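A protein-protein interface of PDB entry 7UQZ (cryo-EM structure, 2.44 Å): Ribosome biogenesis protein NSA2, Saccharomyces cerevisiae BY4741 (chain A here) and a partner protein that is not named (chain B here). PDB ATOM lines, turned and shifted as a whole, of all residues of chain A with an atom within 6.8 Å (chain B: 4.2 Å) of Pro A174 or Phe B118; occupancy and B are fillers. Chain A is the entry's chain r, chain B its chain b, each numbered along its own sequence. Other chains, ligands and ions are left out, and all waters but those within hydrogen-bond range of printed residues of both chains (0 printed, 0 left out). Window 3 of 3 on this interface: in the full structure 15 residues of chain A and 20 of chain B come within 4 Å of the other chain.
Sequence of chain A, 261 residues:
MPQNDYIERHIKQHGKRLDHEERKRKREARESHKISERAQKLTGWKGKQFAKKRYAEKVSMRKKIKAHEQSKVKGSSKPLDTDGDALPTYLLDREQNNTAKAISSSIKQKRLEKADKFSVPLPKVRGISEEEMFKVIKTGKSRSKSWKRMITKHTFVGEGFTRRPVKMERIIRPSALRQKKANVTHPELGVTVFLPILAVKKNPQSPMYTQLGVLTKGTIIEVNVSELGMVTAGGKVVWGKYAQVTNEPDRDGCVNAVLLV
Among the printed residues, merely in contact across the chains: Ala A176 with Leu B115, Thr A152 with Gln B120, Ala A176 with Phe B118, Ala A176 with Arg B114, Pro A174 with Phe B118 and Leu A177 with Leu B115.
Of the 14 printed residues of chain A, 4 touch a printed residue of chain B. Hydrophobic or aromatic side chains of chain B that line the printed part of chain A: Leu B115 and Phe B118. Among the printed residues, 6 pairs touch across the chains. Among the printed residues, no Asp or Glu carboxylate lies within 4 Å of a Lys or Arg side-chain nitrogen of the other chain.
The backbone NH (N) of Thr A155 sits at hydrogen-bond distance from the backbone carbonyl oxygen (O) of Leu A177.
Printed residues of chain A within 4 Å of Arg B114: Ala A176 (3.8 Å). Of the printed residues of chain B, Thr A152 touches Gln B120. Printed residues of chain A within 4 Å of Gln B120: Thr A152. Printed residues of chain B within 4 Å of Leu A177: Leu B115. Met A150 touches none of the printed residues of chain B.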
ATOM      1  N   MET A 150     -22.755 -14.207  14.909  1.00  0.00           N
ATOM      2  CA  MET A 150     -21.366 -13.920  15.246  1.00  0.00           C
ATOM      3  C   MET A 150     -21.244 -13.646  16.738  1.00  0.00           C
ATOM      4  O   MET A 150     -22.020 -12.861  17.294  1.00  0.00           O
ATOM      5  CB  MET A 150     -20.841 -12.719  14.456  1.00  0.00           C
ATOM      6  CG  MET A 150     -19.350 -12.474  14.642  1.00  0.00           C
ATOM      7  SD  MET A 150     -18.755 -10.951  13.890  1.00  0.00           S
ATOM      8  CE  MET A 150     -19.473  -9.732  14.982  1.00  0.00           C
ATOM      9  N   ILE A 151     -20.276 -14.289  17.382  1.00  0.00           N
ATOM     10  CA  ILE A 151     -20.030 -14.075  18.805  1.00  0.00           C
ATOM     11  C   ILE A 151     -19.224 -12.794  18.973  1.00  0.00           C
ATOM     12  O   ILE A 151     -18.139 -12.648  18.398  1.00  0.00           O
ATOM     13  CB  ILE A 151     -19.304 -15.275  19.429  1.00  0.00           C
ATOM     14  CG1 ILE A 151     -20.209 -16.509  19.410  1.00  0.00           C
ATOM     15  CG2 ILE A 151     -18.855 -14.954  20.845  1.00  0.00           C
ATOM     16  CD1 ILE A 151     -19.575 -17.749  19.991  1.00  0.00           C
ATOM     17  N   THR A 152     -19.751 -11.862  19.766  1.00  0.00           N
ATOM     18  CA  THR A 152     -19.124 -10.562  19.962  1.00  0.00           C
ATOM     19  C   THR A 152     -18.131 -10.537  21.116  1.00  0.00           C
ATOM     20  O   THR A 152     -17.440  -9.528  21.293  1.00  0.00           O
ATOM     21  CB  THR A 152     -20.196  -9.493  20.198  1.00  0.00           C
ATOM     22  OG1 THR A 152     -20.944  -9.817  21.375  1.00  0.00           O
ATOM     23  CG2 THR A 152     -21.143  -9.416  19.010  1.00  0.00           C
ATOM     24  N   LYS A 153     -18.040 -11.606  21.899  1.00  0.00           N
ATOM     25  CA  LYS A 153     -17.116 -11.679  23.020  1.00  0.00           C
ATOM     26  C   LYS A 153     -15.855 -12.442  22.621  1.00  0.00           C
ATOM     27  O   LYS A 153     -15.788 -13.084  21.571  1.00  0.00           O
ATOM     28  CB  LYS A 153     -17.788 -12.346  24.225  1.00  0.00           C
ATOM     29  CG  LYS A 153     -19.061 -11.665  24.693  1.00  0.00           C
ATOM     30  CD  LYS A 153     -18.821 -10.202  25.012  1.00  0.00           C
ATOM     31  CE  LYS A 153     -19.934  -9.626  25.869  1.00  0.00           C
ATOM     32  NZ  LYS A 153     -21.258  -9.682  25.198  1.00  0.00           N
ATOM     33  N   THR A 155     -13.112 -15.385  22.724  1.00  0.00           N
ATOM     34  CA  THR A 155     -13.284 -16.828  22.788  1.00  0.00           C
ATOM     35  C   THR A 155     -11.932 -17.521  22.875  1.00  0.00           C
ATOM     36  O   THR A 155     -10.886 -16.946  22.565  1.00  0.00           O
ATOM     37  CB  THR A 155     -14.053 -17.369  21.569  1.00  0.00           C
ATOM     38  OG1 THR A 155     -13.365 -17.009  20.365  1.00  0.00           O
ATOM     39  CG2 THR A 155     -15.468 -16.812  21.528  1.00  0.00           C
ATOM     40  N   VAL A 157     -10.509 -21.137  21.342  1.00  0.00           N
ATOM     41  CA  VAL A 157     -10.881 -22.180  20.390  1.00  0.00           C
ATOM     42  C   VAL A 157     -10.039 -23.443  20.520  1.00  0.00           C
ATOM     43  O   VAL A 157     -10.293 -24.416  19.794  1.00  0.00           O
ATOM     44  CB  VAL A 157     -10.810 -21.660  18.938  1.00  0.00           C
ATOM     45  CG1 VAL A 157     -11.843 -20.570  18.715  1.00  0.00           C
ATOM     46  CG2 VAL A 157      -9.414 -21.149  18.625  1.00  0.00           C
ATOM     47  N   GLU A 169     -21.277 -22.927   8.266  1.00  0.00           N
ATOM     48  CA  GLU A 169     -20.825 -22.195   9.448  1.00  0.00           C
ATOM     49  C   GLU A 169     -21.962 -21.317   9.957  1.00  0.00           C
ATOM     50  O   GLU A 169     -22.236 -20.251   9.402  1.00  0.00           O
ATOM     51  CB  GLU A 169     -19.592 -21.361   9.122  1.00  0.00           C
ATOM     52  CG  GLU A 169     -18.984 -20.655  10.324  1.00  0.00           C
ATOM     53  CD  GLU A 169     -18.000 -19.571   9.931  1.00  0.00           C
ATOM     54  OE1 GLU A 169     -18.068 -19.091   8.782  1.00  0.00           O
ATOM     55  OE2 GLU A 169     -17.159 -19.198  10.773  1.00  0.00           O
ATOM     56  N   ILE A 172     -20.096 -18.032  14.344  1.00  0.00           N
ATOM     57  CA  ILE A 172     -18.882 -17.417  13.826  1.00  0.00           C
ATOM     58  C   ILE A 172     -18.090 -16.851  14.994  1.00  0.00           C
ATOM     59  O   ILE A 172     -18.592 -15.998  15.739  1.00  0.00           O
ATOM     60  CB  ILE A 172     -19.194 -16.317  12.799  1.00  0.00           C
ATOM     61  CG1 ILE A 172     -19.906 -16.907  11.580  1.00  0.00           C
ATOM     62  CG2 ILE A 172     -17.922 -15.592  12.396  1.00  0.00           C
ATOM     63  CD1 ILE A 172     -20.404 -15.864  10.609  1.00  0.00           C
ATOM     64  N   ARG A 173     -16.855 -17.314  15.143  1.00  0.00           N
ATOM     65  CA  ARG A 173     -15.917 -16.781  16.130  1.00  0.00           C
ATOM     66  C   ARG A 173     -14.770 -16.123  15.380  1.00  0.00           C
ATOM     67  O   ARG A 173     -13.869 -16.822  14.884  1.00  0.00           O
ATOM     68  CB  ARG A 173     -15.402 -17.886  17.049  1.00  0.00           C
ATOM     69  CG  ARG A 173     -16.451 -18.430  17.998  1.00  0.00           C
ATOM     70  CD  ARG A 173     -15.980 -19.686  18.710  1.00  0.00           C
ATOM     71  NE  ARG A 173     -16.013 -20.854  17.838  1.00  0.00           N
ATOM     72  CZ  ARG A 173     -15.873 -22.104  18.257  1.00  0.00           C
ATOM     73  NH1 ARG A 173     -15.689 -22.389  19.535  1.00  0.00           N
ATOM     74  NH2 ARG A 173     -15.935 -23.095  17.374  1.00  0.00           N
ATOM     75  N   PRO A 174     -14.766 -14.795  15.245  1.00  0.00           N
ATOM     76  CA  PRO A 174     -13.717 -14.136  14.461  1.00  0.00           C
ATOM     77  C   PRO A 174     -12.345 -14.286  15.099  1.00  0.00           C
ATOM     78  O   PRO A 174     -12.207 -14.374  16.321  1.00  0.00           O
ATOM     79  CB  PRO A 174     -14.165 -12.670  14.424  1.00  0.00           C
ATOM     80  CG  PRO A 174     -15.094 -12.522  15.571  1.00  0.00           C
ATOM     81  CD  PRO A 174     -15.773 -13.841  15.738  1.00  0.00           C
ATOM     82  N   SER A 175     -11.322 -14.312  14.241  1.00  0.00           N
ATOM     83  CA  SER A 175      -9.964 -14.601  14.690  1.00  0.00           C
ATOM     84  C   SER A 175      -9.405 -13.501  15.583  1.00  0.00           C
ATOM     85  O   SER A 175      -8.621 -13.790  16.493  1.00  0.00           O
ATOM     86  CB  SER A 175      -9.052 -14.825  13.485  1.00  0.00           C
ATOM     87  OG  SER A 175      -9.205 -13.792  12.532  1.00  0.00           O
ATOM     88  N   ALA A 176      -9.786 -12.243  15.342  1.00  0.00           N
ATOM     89  CA  ALA A 176      -9.294 -11.140  16.161  1.00  0.00           C
ATOM     90  C   ALA A 176      -9.764 -11.232  17.607  1.00  0.00           C
ATOM     91  O   ALA A 176      -9.125 -10.650  18.489  1.00  0.00           O
ATOM     92  CB  ALA A 176      -9.726  -9.802  15.563  1.00  0.00           C
ATOM     93  N   LEU A 177     -10.856 -11.943  17.870  1.00  0.00           N
ATOM     94  CA  LEU A 177     -11.377 -12.106  19.219  1.00  0.00           C
ATOM     95  C   LEU A 177     -10.898 -13.384  19.894  1.00  0.00           C
ATOM     96  O   LEU A 177     -11.317 -13.665  21.019  1.00  0.00           O
ATOM     97  CB  LEU A 177     -12.909 -12.068  19.198  1.00  0.00           C
ATOM     98  CG  LEU A 177     -13.547 -10.802  18.615  1.00  0.00           C
ATOM     99  CD1 LEU A 177     -15.054 -10.801  18.821  1.00  0.00           C
ATOM    100  CD2 LEU A 177     -12.924  -9.550  19.214  1.00  0.00           C
ATOM    101  N   ARG A 178     -10.037 -14.163  19.242  1.00  0.00           N
ATOM    102  CA  ARG A 178      -9.537 -15.400  19.827  1.00  0.00           C
ATOM    103  C   ARG A 178      -8.324 -15.128  20.707  1.00  0.00           C
ATOM    104  O   ARG A 178      -7.392 -14.426  20.309  1.00  0.00           O
ATOM    105  CB  ARG A 178      -9.172 -16.404  18.733  1.00  0.00           C
ATOM    106  CG  ARG A 178     -10.325 -16.785  17.826  1.00  0.00           C
ATOM    107  CD  ARG A 178      -9.860 -17.687  16.695  1.00  0.00           C
ATOM    108  NE  ARG A 178     -10.845 -17.781  15.626  1.00  0.00           N
ATOM    109  CZ  ARG A 178     -10.602 -18.301  14.431  1.00  0.00           C
ATOM    110  NH1 ARG A 178      -9.414 -18.794  14.121  1.00  0.00           N
ATOM    111  NH2 ARG A 178     -11.572 -18.319  13.522  1.00  0.00           N
ATOM    112  N   ARG B 114      -7.677  -3.217  15.406  1.00  0.00           N
ATOM    113  CA  ARG B 114      -8.326  -4.466  15.017  1.00  0.00           C
ATOM    114  C   ARG B 114      -9.459  -4.827  15.973  1.00  0.00           C
ATOM    115  O   ARG B 114     -10.513  -5.306  15.541  1.00  0.00           O
ATOM    116  CB  ARG B 114      -7.297  -5.593  14.953  1.00  0.00           C
ATOM    117  CG  ARG B 114      -7.735  -6.782  14.118  1.00  0.00           C
ATOM    118  CD  ARG B 114      -6.707  -7.903  14.145  1.00  0.00           C
ATOM    119  NE  ARG B 114      -5.378  -7.440  13.766  1.00  0.00           N
ATOM    120  CZ  ARG B 114      -4.358  -7.315  14.606  1.00  0.00           C
ATOM    121  NH1 ARG B 114      -4.474  -7.631  15.884  1.00  0.00           N
ATOM    122  NH2 ARG B 114      -3.196  -6.858  14.150  1.00  0.00           N
ATOM    123  N   LEU B 115      -9.264  -4.602  17.275  1.00  0.00           N
ATOM    124  CA  LEU B 115     -10.335  -4.863  18.235  1.00  0.00           C
ATOM    125  C   LEU B 115     -11.484  -3.872  18.081  1.00  0.00           C
ATOM    126  O   LEU B 115     -12.655  -4.254  18.196  1.00  0.00           O
ATOM    127  CB  LEU B 115      -9.793  -4.831  19.662  1.00  0.00           C
ATOM    128  CG  LEU B 115      -8.936  -6.022  20.090  1.00  0.00           C
ATOM    129  CD1 LEU B 115      -8.479  -5.843  21.520  1.00  0.00           C
ATOM    130  CD2 LEU B 115      -9.701  -7.324  19.925  1.00  0.00           C
ATOM    131  N   LEU B 116     -11.176  -2.597  17.820  1.00  0.00           N
ATOM    132  CA  LEU B 116     -12.215  -1.594  17.614  1.00  0.00           C
ATOM    133  C   LEU B 116     -13.048  -1.874  16.377  1.00  0.00           C
ATOM    134  O   LEU B 116     -14.154  -1.339  16.258  1.00  0.00           O
ATOM    135  CB  LEU B 116     -11.597  -0.201  17.503  1.00  0.00           C
ATOM    136  CG  LEU B 116     -11.362   0.572  18.798  1.00  0.00           C
ATOM    137  CD1 LEU B 116     -10.580   1.837  18.512  1.00  0.00           C
ATOM    138  CD2 LEU B 116     -12.686   0.896  19.470  1.00  0.00           C
ATOM    139  N   LYS B 117     -12.537  -2.681  15.444  1.00  0.00           N
ATOM    140  CA  LYS B 117     -13.368  -3.114  14.322  1.00  0.00           C
ATOM    141  C   LYS B 117     -14.622  -3.871  14.761  1.00  0.00           C
ATOM    142  O   LYS B 117     -15.596  -3.918  14.004  1.00  0.00           O
ATOM    143  CB  LYS B 117     -12.567  -3.997  13.366  1.00  0.00           C
ATOM    144  CG  LYS B 117     -11.621  -3.245  12.454  1.00  0.00           C
ATOM    145  CD  LYS B 117     -10.672  -4.205  11.758  1.00  0.00           C
ATOM    146  CE  LYS B 117     -11.425  -5.321  11.058  1.00  0.00           C
ATOM    147  NZ  LYS B 117     -10.499  -6.324  10.467  1.00  0.00           N
ATOM    148  N   PHE B 118     -14.628  -4.463  15.958  1.00  0.00           N
ATOM    149  CA  PHE B 118     -15.746  -5.279  16.420  1.00  0.00           C
ATOM    150  C   PHE B 118     -16.493  -4.653  17.595  1.00  0.00           C
ATOM    151  O   PHE B 118     -17.164  -5.371  18.343  1.00  0.00           O
ATOM    152  CB  PHE B 118     -15.260  -6.678  16.800  1.00  0.00           C
ATOM    153  CG  PHE B 118     -14.731  -7.471  15.642  1.00  0.00           C
ATOM    154  CD1 PHE B 118     -15.584  -8.227  14.858  1.00  0.00           C
ATOM    155  CD2 PHE B 118     -13.383  -7.459  15.337  1.00  0.00           C
ATOM    156  CE1 PHE B 118     -15.101  -8.956  13.792  1.00  0.00           C
ATOM    157  CE2 PHE B 118     -12.894  -8.186  14.271  1.00  0.00           C
ATOM    158  CZ  PHE B 118     -13.755  -8.937  13.499  1.00  0.00           C
ATOM    159  N   GLY B 119     -16.393  -3.340  17.775  1.00  0.00           N
ATOM    160  CA  GLY B 119     -17.114  -2.694  18.860  1.00  0.00           C
ATOM    161  C   GLY B 119     -18.607  -2.642  18.579  1.00  0.00           C
ATOM    162  O   GLY B 119     -19.043  -2.421  17.449  1.00  0.00           O
ATOM    163  N   GLN B 120     -19.400  -2.846  19.631  1.00  0.00           N
ATOM    164  CA  GLN B 120     -20.849  -2.907  19.499  1.00  0.00           C
ATOM    165  C   GLN B 120     -21.573  -1.711  20.098  1.00  0.00           C
ATOM    166  O   GLN B 120     -22.776  -1.563  19.867  1.00  0.00           O
ATOM    167  CB  GLN B 120     -21.392  -4.193  20.144  1.00  0.00           C
ATOM    168  CG  GLN B 120     -20.916  -5.473  19.481  1.00  0.00           C
ATOM    169  CD  GLN B 120     -21.377  -5.592  18.043  1.00  0.00           C
ATOM    170  OE1 GLN B 120     -22.456  -5.123  17.685  1.00  0.00           O
ATOM    171  NE2 GLN B 120     -20.558  -6.221  17.210  1.00  0.00           N
